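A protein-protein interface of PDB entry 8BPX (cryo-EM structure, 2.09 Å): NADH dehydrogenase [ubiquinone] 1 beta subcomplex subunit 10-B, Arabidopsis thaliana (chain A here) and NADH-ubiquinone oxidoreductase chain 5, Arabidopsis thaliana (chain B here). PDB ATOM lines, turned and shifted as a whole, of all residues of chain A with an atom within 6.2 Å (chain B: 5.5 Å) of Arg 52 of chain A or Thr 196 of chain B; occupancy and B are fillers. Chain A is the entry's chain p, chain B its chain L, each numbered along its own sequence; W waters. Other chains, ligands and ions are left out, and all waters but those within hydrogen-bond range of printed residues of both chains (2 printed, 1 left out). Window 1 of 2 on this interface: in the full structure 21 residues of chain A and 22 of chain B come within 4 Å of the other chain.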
ATOM      1  N   LYS A  47     -28.689   8.117 -19.677  1.00  0.00           N
ATOM      2  CA  LYS A  47     -29.521   9.353 -19.590  1.00  0.00           C
ATOM      3  C   LYS A  47     -28.687  10.510 -19.054  1.00  0.00           C
ATOM      4  O   LYS A  47     -28.663  11.533 -19.733  1.00  0.00           O
ATOM      5  CB  LYS A  47     -30.796   9.144 -18.770  1.00  0.00           C
ATOM      6  CG  LYS A  47     -32.015   8.615 -19.487  1.00  0.00           C
ATOM      7  CD  LYS A  47     -33.207   8.817 -18.598  1.00  0.00           C
ATOM      8  CE  LYS A  47     -34.135   7.633 -18.525  1.00  0.00           C
ATOM      9  NZ  LYS A  47     -35.008   7.552 -19.710  1.00  0.00           N
ATOM     10  N   ALA A  48     -27.981  10.325 -17.928  1.00  0.00           N
ATOM     11  CA  ALA A  48     -27.076  11.365 -17.434  1.00  0.00           C
ATOM     12  C   ALA A  48     -25.997  11.745 -18.497  1.00  0.00           C
ATOM     13  O   ALA A  48     -25.720  12.903 -18.610  1.00  0.00           O
ATOM     14  CB  ALA A  48     -26.538  11.026 -16.056  1.00  0.00           C
ATOM     15  N   LYS A  49     -25.523  10.811 -19.311  1.00  0.00           N
ATOM     16  CA  LYS A  49     -24.487  11.074 -20.334  1.00  0.00           C
ATOM     17  C   LYS A  49     -25.081  11.914 -21.472  1.00  0.00           C
ATOM     18  O   LYS A  49     -24.385  12.762 -21.982  1.00  0.00           O
ATOM     19  CB  LYS A  49     -23.814   9.776 -20.796  1.00  0.00           C
ATOM     20  CG  LYS A  49     -23.225   8.935 -19.680  1.00  0.00           C
ATOM     21  CD  LYS A  49     -21.772   8.625 -19.829  1.00  0.00           C
ATOM     22  CE  LYS A  49     -21.390   8.013 -21.154  1.00  0.00           C
ATOM     23  NZ  LYS A  49     -22.094   6.742 -21.391  1.00  0.00           N
ATOM     24  N   ILE A  50     -26.306  11.602 -21.841  1.00  0.00           N
ATOM     25  CA  ILE A  50     -27.037  12.386 -22.861  1.00  0.00           C
ATOM     26  C   ILE A  50     -27.273  13.829 -22.348  1.00  0.00           C
ATOM     27  O   ILE A  50     -26.923  14.719 -23.093  1.00  0.00           O
ATOM     28  CB  ILE A  50     -28.295  11.636 -23.341  1.00  0.00           C
ATOM     29  CG1 ILE A  50     -27.947  10.418 -24.193  1.00  0.00           C
ATOM     30  CG2 ILE A  50     -29.257  12.560 -24.076  1.00  0.00           C
ATOM     31  CD1 ILE A  50     -28.983   9.343 -24.154  1.00  0.00           C
ATOM     32  N   LEU A  51     -27.710  14.005 -21.110  1.00  0.00           N
ATOM     33  CA  LEU A  51     -27.896  15.334 -20.525  1.00  0.00           C
ATOM     34  C   LEU A  51     -26.574  16.091 -20.443  1.00  0.00           C
ATOM     35  O   LEU A  51     -26.525  17.307 -20.674  1.00  0.00           O
ATOM     36  CB  LEU A  51     -28.536  15.220 -19.143  1.00  0.00           C
ATOM     37  CG  LEU A  51     -30.011  14.815 -19.092  1.00  0.00           C
ATOM     38  CD1 LEU A  51     -30.501  14.732 -17.656  1.00  0.00           C
ATOM     39  CD2 LEU A  51     -30.875  15.757 -19.910  1.00  0.00           C
ATOM     40  N   ARG A  52     -25.443  15.425 -20.214  1.00  0.00           N
ATOM     41  CA  ARG A  52     -24.102  16.055 -20.172  1.00  0.00           C
ATOM     42  C   ARG A  52     -23.727  16.651 -21.562  1.00  0.00           C
ATOM     43  O   ARG A  52     -23.188  17.731 -21.559  1.00  0.00           O
ATOM     44  CB  ARG A  52     -23.078  15.092 -19.555  1.00  0.00           C
ATOM     45  CG  ARG A  52     -21.648  15.587 -19.458  1.00  0.00           C
ATOM     46  CD  ARG A  52     -20.883  14.619 -18.588  1.00  0.00           C
ATOM     47  NE  ARG A  52     -20.623  13.359 -19.255  1.00  0.00           N
ATOM     48  CZ  ARG A  52     -20.189  12.273 -18.650  1.00  0.00           C
ATOM     49  NH1 ARG A  52     -19.986  12.281 -17.350  1.00  0.00           N
ATOM     50  NH2 ARG A  52     -19.960  11.184 -19.344  1.00  0.00           N
ATOM     51  N   GLU A  53     -23.968  15.947 -22.637  1.00  0.00           N
ATOM     52  CA  GLU A  53     -23.763  16.447 -24.032  1.00  0.00           C
ATOM     53  C   GLU A  53     -24.530  17.799 -24.251  1.00  0.00           C
ATOM     54  O   GLU A  53     -23.885  18.692 -24.719  1.00  0.00           O
ATOM     55  CB  GLU A  53     -24.059  15.321 -25.034  1.00  0.00           C
ATOM     56  CG  GLU A  53     -23.011  15.198 -26.094  1.00  0.00           C
ATOM     57  CD  GLU A  53     -21.616  14.995 -25.539  1.00  0.00           C
ATOM     58  OE1 GLU A  53     -21.472  14.237 -24.573  1.00  0.00           O
ATOM     59  OE2 GLU A  53     -20.689  15.618 -26.063  1.00  0.00           O
ATOM     60  N   LYS A  54     -25.761  17.931 -23.739  1.00  0.00           N
ATOM     61  CA  LYS A  54     -26.559  19.223 -23.782  1.00  0.00           C
ATOM     62  C   LYS A  54     -25.832  20.380 -23.092  1.00  0.00           C
ATOM     63  O   LYS A  54     -25.587  21.323 -23.758  1.00  0.00           O
ATOM     64  CB  LYS A  54     -27.985  18.963 -23.280  1.00  0.00           C
ATOM     65  CG  LYS A  54     -28.769  17.945 -24.099  1.00  0.00           C
ATOM     66  CD  LYS A  54     -30.208  17.797 -23.662  1.00  0.00           C
ATOM     67  CE  LYS A  54     -30.846  16.469 -23.997  1.00  0.00           C
ATOM     68  NZ  LYS A  54     -30.717  16.090 -25.421  1.00  0.00           N
ATOM     69  N   VAL A  55     -25.345  20.159 -21.869  1.00  0.00           N
ATOM     70  CA  VAL A  55     -24.585  21.155 -21.092  1.00  0.00           C
ATOM     71  C   VAL A  55     -23.327  21.503 -21.847  1.00  0.00           C
ATOM     72  O   VAL A  55     -23.143  22.687 -22.014  1.00  0.00           O
ATOM     73  CB  VAL A  55     -24.347  20.709 -19.628  1.00  0.00           C
ATOM     74  CG1 VAL A  55     -23.429  21.623 -18.857  1.00  0.00           C
ATOM     75  CG2 VAL A  55     -25.654  20.481 -18.891  1.00  0.00           C
ATOM     76  N   LYS A  56     -22.562  20.492 -22.284  1.00  0.00           N
ATOM     77  CA  LYS A  56     -21.304  20.692 -22.987  1.00  0.00           C
ATOM     78  C   LYS A  56     -21.559  21.726 -24.111  1.00  0.00           C
ATOM     79  O   LYS A  56     -20.925  22.756 -24.086  1.00  0.00           O
ATOM     80  CB  LYS A  56     -20.730  19.360 -23.514  1.00  0.00           C
ATOM     81  CG  LYS A  56     -19.371  19.390 -24.182  1.00  0.00           C
ATOM     82  CD  LYS A  56     -18.926  18.046 -24.725  1.00  0.00           C
ATOM     83  CE  LYS A  56     -18.559  17.022 -23.671  1.00  0.00           C
ATOM     84  NZ  LYS A  56     -19.672  16.121 -23.290  1.00  0.00           N
ATOM     85  N   TRP A  57     -22.515  21.431 -24.955  1.00  0.00           N
ATOM     86  CA  TRP A  57     -22.824  22.262 -26.145  1.00  0.00           C
ATOM     87  C   TRP A  57     -23.437  23.618 -25.811  1.00  0.00           C
ATOM     88  O   TRP A  57     -23.023  24.516 -26.456  1.00  0.00           O
ATOM     89  CB  TRP A  57     -23.592  21.439 -27.167  1.00  0.00           C
ATOM     90  CG  TRP A  57     -22.620  20.496 -27.805  1.00  0.00           C
ATOM     91  CD1 TRP A  57     -22.564  19.142 -27.654  1.00  0.00           C
ATOM     92  CD2 TRP A  57     -21.473  20.856 -28.595  1.00  0.00           C
ATOM     93  NE1 TRP A  57     -21.497  18.636 -28.336  1.00  0.00           N
ATOM     94  CE2 TRP A  57     -20.811  19.656 -28.931  1.00  0.00           C
ATOM     95  CE3 TRP A  57     -20.956  22.064 -29.075  1.00  0.00           C
ATOM     96  CZ2 TRP A  57     -19.659  19.629 -29.712  1.00  0.00           C
ATOM     97  CZ3 TRP A  57     -19.820  22.037 -29.848  1.00  0.00           C
ATOM     98  CH2 TRP A  57     -19.186  20.834 -30.174  1.00  0.00           C
ATOM     99  N   TYR A  59     -22.837  25.474 -22.972  1.00  0.00           N
ATOM    100  CA  TYR A  59     -21.624  26.196 -22.564  1.00  0.00           C
ATOM    101  C   TYR A  59     -20.905  26.700 -23.808  1.00  0.00           C
ATOM    102  O   TYR A  59     -20.664  27.877 -23.821  1.00  0.00           O
ATOM    103  CB  TYR A  59     -20.702  25.396 -21.621  1.00  0.00           C
ATOM    104  CG  TYR A  59     -19.556  26.132 -21.005  1.00  0.00           C
ATOM    105  CD1 TYR A  59     -19.727  26.804 -19.810  1.00  0.00           C
ATOM    106  CD2 TYR A  59     -18.309  26.127 -21.602  1.00  0.00           C
ATOM    107  CE1 TYR A  59     -18.680  27.466 -19.219  1.00  0.00           C
ATOM    108  CE2 TYR A  59     -17.246  26.785 -21.018  1.00  0.00           C
ATOM    109  CZ  TYR A  59     -17.441  27.457 -19.828  1.00  0.00           C
ATOM    110  OH  TYR A  59     -16.433  28.121 -19.220  1.00  0.00           O
ATOM    111  N   VAL A  74     -28.343  22.479 -16.735  1.00  0.00           N
ATOM    112  CA  VAL A  74     -27.450  22.180 -15.622  1.00  0.00           C
ATOM    113  C   VAL A  74     -28.228  21.537 -14.484  1.00  0.00           C
ATOM    114  O   VAL A  74     -27.775  20.556 -13.880  1.00  0.00           O
ATOM    115  CB  VAL A  74     -26.716  23.452 -15.159  1.00  0.00           C
ATOM    116  CG1 VAL A  74     -26.033  23.219 -13.819  1.00  0.00           C
ATOM    117  CG2 VAL A  74     -25.712  23.897 -16.201  1.00  0.00           C
ATOM    118  N   TYR A  77     -29.049  17.908 -15.474  1.00  0.00           N
ATOM    119  CA  TYR A  77     -27.883  17.035 -15.419  1.00  0.00           C
ATOM    120  C   TYR A  77     -27.483  16.735 -13.982  1.00  0.00           C
ATOM    121  O   TYR A  77     -27.198  15.584 -13.640  1.00  0.00           O
ATOM    122  CB  TYR A  77     -26.702  17.652 -16.165  1.00  0.00           C
ATOM    123  CG  TYR A  77     -25.408  16.922 -15.885  1.00  0.00           C
ATOM    124  CD1 TYR A  77     -25.191  15.648 -16.396  1.00  0.00           C
ATOM    125  CD2 TYR A  77     -24.426  17.479 -15.078  1.00  0.00           C
ATOM    126  CE1 TYR A  77     -24.029  14.967 -16.135  1.00  0.00           C
ATOM    127  CE2 TYR A  77     -23.258  16.801 -14.808  1.00  0.00           C
ATOM    128  CZ  TYR A  77     -23.065  15.539 -15.345  1.00  0.00           C
ATOM    129  OH  TYR A  77     -21.910  14.844 -15.091  1.00  0.00           O
ATOM    130  N   GLU B  68     -18.496   3.780 -17.105  1.00  0.00           N
ATOM    131  CA  GLU B  68     -19.723   4.372 -16.502  1.00  0.00           C
ATOM    132  C   GLU B  68     -19.698   5.887 -16.754  1.00  0.00           C
ATOM    133  O   GLU B  68     -19.541   6.283 -17.920  1.00  0.00           O
ATOM    134  CB  GLU B  68     -19.802   4.010 -15.014  1.00  0.00           C
ATOM    135  CG  GLU B  68     -21.190   4.118 -14.417  1.00  0.00           C
ATOM    136  CD  GLU B  68     -21.215   4.469 -12.939  1.00  0.00           C
ATOM    137  OE1 GLU B  68     -21.320   3.542 -12.114  1.00  0.00           O
ATOM    138  OE2 GLU B  68     -21.133   5.671 -12.619  1.00  0.00           O
ATOM    139  N   MET B  69     -19.840   6.701 -15.707  1.00  0.00           N
ATOM    140  CA  MET B  69     -19.787   8.195 -15.831  1.00  0.00           C
ATOM    141  C   MET B  69     -18.388   8.732 -16.203  1.00  0.00           C
ATOM    142  O   MET B  69     -18.365   9.752 -16.841  1.00  0.00           O
ATOM    143  CB  MET B  69     -20.345   8.940 -14.611  1.00  0.00           C
ATOM    144  CG  MET B  69     -21.789   8.648 -14.301  1.00  0.00           C
ATOM    145  SD  MET B  69     -22.901   9.082 -15.642  1.00  0.00           S
ATOM    146  CE  MET B  69     -22.723  10.865 -15.694  1.00  0.00           C
ATOM    147  N   PHE B  70     -17.290   8.060 -15.856  1.00  0.00           N
ATOM    148  CA  PHE B  70     -15.891   8.528 -16.156  1.00  0.00           C
ATOM    149  C   PHE B  70     -15.733   8.637 -17.681  1.00  0.00           C
ATOM    150  O   PHE B  70     -15.876   7.670 -18.371  1.00  0.00           O
ATOM    151  CB  PHE B  70     -14.891   7.871 -15.191  1.00  0.00           C
ATOM    152  CG  PHE B  70     -13.515   8.477 -15.142  1.00  0.00           C
ATOM    153  CD1 PHE B  70     -13.196   9.437 -14.195  1.00  0.00           C
ATOM    154  CD2 PHE B  70     -12.534   8.066 -16.028  1.00  0.00           C
ATOM    155  CE1 PHE B  70     -11.924   9.980 -14.143  1.00  0.00           C
ATOM    156  CE2 PHE B  70     -11.262   8.614 -15.981  1.00  0.00           C
ATOM    157  CZ  PHE B  70     -10.957   9.559 -15.030  1.00  0.00           C
ATOM    158  N   ASP B  71     -15.422   9.837 -18.181  1.00  0.00           N
ATOM    159  CA  ASP B  71     -15.556  10.162 -19.598  1.00  0.00           C
ATOM    160  C   ASP B  71     -14.308  10.831 -20.158  1.00  0.00           C
ATOM    161  O   ASP B  71     -14.395  11.757 -20.967  1.00  0.00           O
ATOM    162  CB  ASP B  71     -16.774  11.057 -19.830  1.00  0.00           C
ATOM    163  CG  ASP B  71     -16.674  12.394 -19.097  1.00  0.00           C
ATOM    164  OD1 ASP B  71     -15.970  12.478 -18.070  1.00  0.00           O
ATOM    165  OD2 ASP B  71     -17.294  13.370 -19.560  1.00  0.00           O
ATOM    166  N   PHE B 186     -14.072  14.792 -10.431  1.00  0.00           N
ATOM    167  CA  PHE B 186     -14.953  13.757 -10.957  1.00  0.00           C
ATOM    168  C   PHE B 186     -16.009  13.357  -9.937  1.00  0.00           C
ATOM    169  O   PHE B 186     -17.167  13.130 -10.291  1.00  0.00           O
ATOM    170  CB  PHE B 186     -14.189  12.509 -11.382  1.00  0.00           C
ATOM    171  CG  PHE B 186     -15.097  11.414 -11.835  1.00  0.00           C
ATOM    172  CD1 PHE B 186     -15.844  11.558 -12.996  1.00  0.00           C
ATOM    173  CD2 PHE B 186     -15.301  10.291 -11.048  1.00  0.00           C
ATOM    174  CE1 PHE B 186     -16.713  10.576 -13.401  1.00  0.00           C
ATOM    175  CE2 PHE B 186     -16.177   9.303 -11.450  1.00  0.00           C
ATOM    176  CZ  PHE B 186     -16.885   9.442 -12.625  1.00  0.00           C
ATOM    177  N   GLN B 190     -19.248  14.235 -11.546  1.00  0.00           N
ATOM    178  CA  GLN B 190     -19.459  13.014 -12.393  1.00  0.00           C
ATOM    179  C   GLN B 190     -18.943  13.266 -13.812  1.00  0.00           C
ATOM    180  O   GLN B 190     -19.468  12.717 -14.714  1.00  0.00           O
ATOM    181  CB  GLN B 190     -20.872  12.445 -12.247  1.00  0.00           C
ATOM    182  CG  GLN B 190     -21.161  11.910 -10.849  1.00  0.00           C
ATOM    183  CD  GLN B 190     -20.380  10.675 -10.470  1.00  0.00           C
ATOM    184  OE1 GLN B 190     -20.580   9.603 -11.017  1.00  0.00           O
ATOM    185  NE2 GLN B 190     -19.492  10.812  -9.502  1.00  0.00           N
ATOM    186  N   THR B 191     -17.896  14.037 -13.951  1.00  0.00           N
ATOM    187  CA  THR B 191     -17.279  14.228 -15.253  1.00  0.00           C
ATOM    188  C   THR B 191     -15.888  14.803 -15.049  1.00  0.00           C
ATOM    189  O   THR B 191     -15.571  15.347 -13.989  1.00  0.00           O
ATOM    190  CB  THR B 191     -18.120  15.146 -16.154  1.00  0.00           C
ATOM    191  OG1 THR B 191     -17.526  15.226 -17.453  1.00  0.00           O
ATOM    192  CG2 THR B 191     -18.223  16.534 -15.559  1.00  0.00           C
ATOM    193  N   ASP B 193     -14.777  16.461 -18.058  1.00  0.00           N
ATOM    194  CA  ASP B 193     -14.879  17.448 -19.180  1.00  0.00           C
ATOM    195  C   ASP B 193     -14.859  18.910 -18.689  1.00  0.00           C
ATOM    196  O   ASP B 193     -15.663  19.275 -17.905  1.00  0.00           O
ATOM    197  CB  ASP B 193     -16.109  17.201 -20.044  1.00  0.00           C
ATOM    198  CG  ASP B 193     -16.271  18.117 -21.223  1.00  0.00           C
ATOM    199  OD1 ASP B 193     -15.743  17.776 -22.273  1.00  0.00           O
ATOM    200  OD2 ASP B 193     -16.923  19.155 -21.072  1.00  0.00           O
ATOM    201  N   PHE B 194     -14.023  19.712 -19.304  1.00  0.00           N
ATOM    202  CA  PHE B 194     -13.879  21.099 -18.862  1.00  0.00           C
ATOM    203  C   PHE B 194     -15.182  21.878 -19.018  1.00  0.00           C
ATOM    204  O   PHE B 194     -15.611  22.574 -18.093  1.00  0.00           O
ATOM    205  CB  PHE B 194     -12.749  21.781 -19.634  1.00  0.00           C
ATOM    206  CG  PHE B 194     -11.378  21.457 -19.116  1.00  0.00           C
ATOM    207  CD1 PHE B 194     -11.175  21.180 -17.770  1.00  0.00           C
ATOM    208  CD2 PHE B 194     -10.293  21.411 -19.974  1.00  0.00           C
ATOM    209  CE1 PHE B 194      -9.910  20.871 -17.292  1.00  0.00           C
ATOM    210  CE2 PHE B 194      -9.031  21.104 -19.501  1.00  0.00           C
ATOM    211  CZ  PHE B 194      -8.842  20.834 -18.160  1.00  0.00           C
ATOM    212  N   SER B 195     -15.828  21.744 -20.172  1.00  0.00           N
ATOM    213  CA  SER B 195     -17.061  22.524 -20.522  1.00  0.00           C
ATOM    214  C   SER B 195     -18.193  22.213 -19.544  1.00  0.00           C
ATOM    215  O   SER B 195     -18.784  23.145 -19.057  1.00  0.00           O
ATOM    216  CB  SER B 195     -17.500  22.414 -22.005  1.00  0.00           C
ATOM    217  OG  SER B 195     -16.431  22.441 -22.898  1.00  0.00           O
ATOM    218  N   THR B 196     -18.362  20.923 -19.221  1.00  0.00           N
ATOM    219  CA  THR B 196     -19.417  20.499 -18.300  1.00  0.00           C
ATOM    220  C   THR B 196     -19.120  21.013 -16.890  1.00  0.00           C
ATOM    221  O   THR B 196     -20.003  21.581 -16.293  1.00  0.00           O
ATOM    222  CB  THR B 196     -19.759  19.007 -18.513  1.00  0.00           C
ATOM    223  OG1 THR B 196     -20.048  18.752 -19.886  1.00  0.00           O
ATOM    224  CG2 THR B 196     -20.872  18.536 -17.604  1.00  0.00           C
ATOM    225  N   ILE B 197     -17.888  20.866 -16.440  1.00  0.00           N
ATOM    226  CA  ILE B 197     -17.524  21.289 -15.092  1.00  0.00           C
ATOM    227  C   ILE B 197     -17.705  22.795 -14.937  1.00  0.00           C
ATOM    228  O   ILE B 197     -18.261  23.267 -13.939  1.00  0.00           O
ATOM    229  CB  ILE B 197     -16.083  20.853 -14.762  1.00  0.00           C
ATOM    230  CG1 ILE B 197     -16.017  19.338 -14.546  1.00  0.00           C
ATOM    231  CG2 ILE B 197     -15.563  21.592 -13.530  1.00  0.00           C
ATOM    232  CD1 ILE B 197     -14.621  18.766 -14.649  1.00  0.00           C
ATOM    233  N   PHE B 198     -17.254  23.570 -15.926  1.00  0.00           N
ATOM    234  CA  PHE B 198     -17.372  25.020 -15.829  1.00  0.00           C
ATOM    235  C   PHE B 198     -18.824  25.472 -15.905  1.00  0.00           C
ATOM    236  O   PHE B 198     -19.189  26.474 -15.283  1.00  0.00           O
ATOM    237  CB  PHE B 198     -16.537  25.705 -16.913  1.00  0.00           C
ATOM    238  CG  PHE B 198     -15.076  25.364 -16.857  1.00  0.00           C
ATOM    239  CD1 PHE B 198     -14.482  24.997 -15.656  1.00  0.00           C
ATOM    240  CD2 PHE B 198     -14.292  25.425 -17.993  1.00  0.00           C
ATOM    241  CE1 PHE B 198     -13.144  24.676 -15.601  1.00  0.00           C
ATOM    242  CE2 PHE B 198     -12.956  25.110 -17.943  1.00  0.00           C
ATOM    243  CZ  PHE B 198     -12.378  24.737 -16.743  1.00  0.00           C
ATOM    244  N   ALA B 199     -19.662  24.748 -16.645  1.00  0.00           N
ATOM    245  CA  ALA B 199     -21.080  25.073 -16.680  1.00  0.00           C
ATOM    246  C   ALA B 199     -21.784  24.767 -15.364  1.00  0.00           C
ATOM    247  O   ALA B 199     -22.815  25.380 -15.072  1.00  0.00           O
ATOM    248  CB  ALA B 199     -21.760  24.322 -17.821  1.00  0.00           C
ATOM    249  N   CYS B 200     -21.247  23.854 -14.557  1.00  0.00           N
ATOM    250  CA  CYS B 200     -21.906  23.405 -13.341  1.00  0.00           C
ATOM    251  C   CYS B 200     -21.326  24.010 -12.070  1.00  0.00           C
ATOM    252  O   CYS B 200     -21.953  23.894 -11.014  1.00  0.00           O
ATOM    253  CB  CYS B 200     -21.830  21.874 -13.231  1.00  0.00           C
ATOM    254  SG  CYS B 200     -22.786  20.946 -14.441  1.00  0.00           S
ATOM    255  N   ALA B 201     -20.164  24.666 -12.147  1.00  0.00           N
ATOM    256  CA  ALA B 201     -19.349  24.913 -10.962  1.00  0.00           C
ATOM    257  C   ALA B 201     -20.000  25.850  -9.953  1.00  0.00           C
ATOM    258  O   ALA B 201     -19.636  25.815  -8.774  1.00  0.00           O
ATOM    259  CB  ALA B 201     -17.986  25.471 -11.370  1.00  0.00           C
HETATM  260  O   HOH W   1     -18.360  14.182 -21.629  1.00  0.00           O
HETATM  261  O   HOH W   2     -20.826   5.112 -19.871  1.00  0.00           O
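Water W1 lies within hydrogen-bond range of OD2 of Asp 71 of chain B (2.5 Å), NZ of Lys 56 of chain A (2.9 Å) and NE of Arg 52 of chain A (3.4 Å). Water W2 lies within hydrogen-bond range of the side-chain amino group (NZ) of Lys 49 of chain A (2.6 Å) and the backbone carbonyl oxygen (O) of Glu 68 of chain B (2.6 Å).
The guanidinium group (NH1) of Arg 52 of chain A sits at hydrogen-bond distance from the backbone carbonyl oxygen (O) of Met 69 of chain B, at 3.0 Å. O of Gln 190 of chain B sits at hydrogen-bond distance from OH of Tyr 77 of chain A (3.3 Å). NH1 of Arg 52 of chain A is in hydrogen-bond range of O of Gln 190 of chain B. NE of Arg 52 of chain A lies within salt-bridge range of OD2 of Asp 71 of chain B.
Of the 14 printed residues of chain A, 8 touch a printed residue of chain B. Of the 16 printed residues of chain B, 11 touch a printed residue of chain A. Hydrophobic or aromatic side chains of chain B within 4 Å of the printed part of chain A: Met 69, Phe 198 and Ala 199. Among the printed residues, Asp or Glu carboxylates within 4 Å of a Lys or Arg side-chain nitrogen of the other chain: Arg 52 of chain A with Asp 71 of chain B (3.3 Å).
The side-chain carboxylate of Asp 193 of chain B sits at hydrogen-bond distance from the backbone NH of Thr 196 of chain B, at 2.9 Å. The backbone carbonyl oxygen (O) of Phe 186 of chain B sits close to the side-chain amide nitrogen (NE2) of Gln 190 of chain B (3.4 Å). The side-chain carboxylate (OE1) of Glu 53 of chain A lies within salt-bridge range of the side-chain amino group (NZ) of Lys 56 of chain A (2.9 Å). OD2 of Asp 193 of chain B sits at hydrogen-bond distance from N of Ser 195 of chain B. OG1 of Thr 191 of chain B lies within hydrogen-bond range of N of Asp 193 of chain B (3.1 Å). OD2 of Asp 71 of chain B sits at hydrogen-bond distance from OG1 of Thr 191 of chain B.
Printed residues of chain A within 4 Å of Thr 196 of chain B: Arg 52 and Lys 56. Of the printed residues of chain B, Ala 48 of chain A touches Met 69 (3.8 Å). Of the printed residues of chain A, Gln 190 of chain B touches Arg 52 and Tyr 77. Lys 54 of chain A touches none of the printed residues of chain B. Glu 53 of chain A touches none of the printed residues of chain B. The nearest residue of chain A that does not touch Thr 196 of chain B is Tyr 77 of chain A (4.1 Å).
Among the printed residues, merely in contact across the chains: Ala 48 of chain A with Met 69 of chain B (3.8 Å), Lys 49 of chain A with Glu 68 of chain B (3.8 Å), Arg 52 of chain A with Thr 191 of chain B (3.6 Å), Arg 52 of chain A with Thr 196 of chain B (3.6 Å), Val 55 of chain A with Ala 199 of chain B (3.3 Å), Lys 56 of chain A with Asp 193 of chain B (3.2 Å), Lys 56 of chain A with Thr 196 of chain B (3.7 Å), Tyr 59 of chain A with Ser 195 of chain B (3.6 Å), Tyr 59 of chain A with Phe 198 of chain B (3.3 Å), Tyr 59 of chain A with Ala 199 of chain B (3.8 Å), Val 74 of chain A with Ala 199 of chain B (3.4 Å), Tyr 77 of chain A with Thr 191 of chain B (3.9 Å) and Tyr 77 of chain A with Cys 200 of chain B (3.9 Å).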
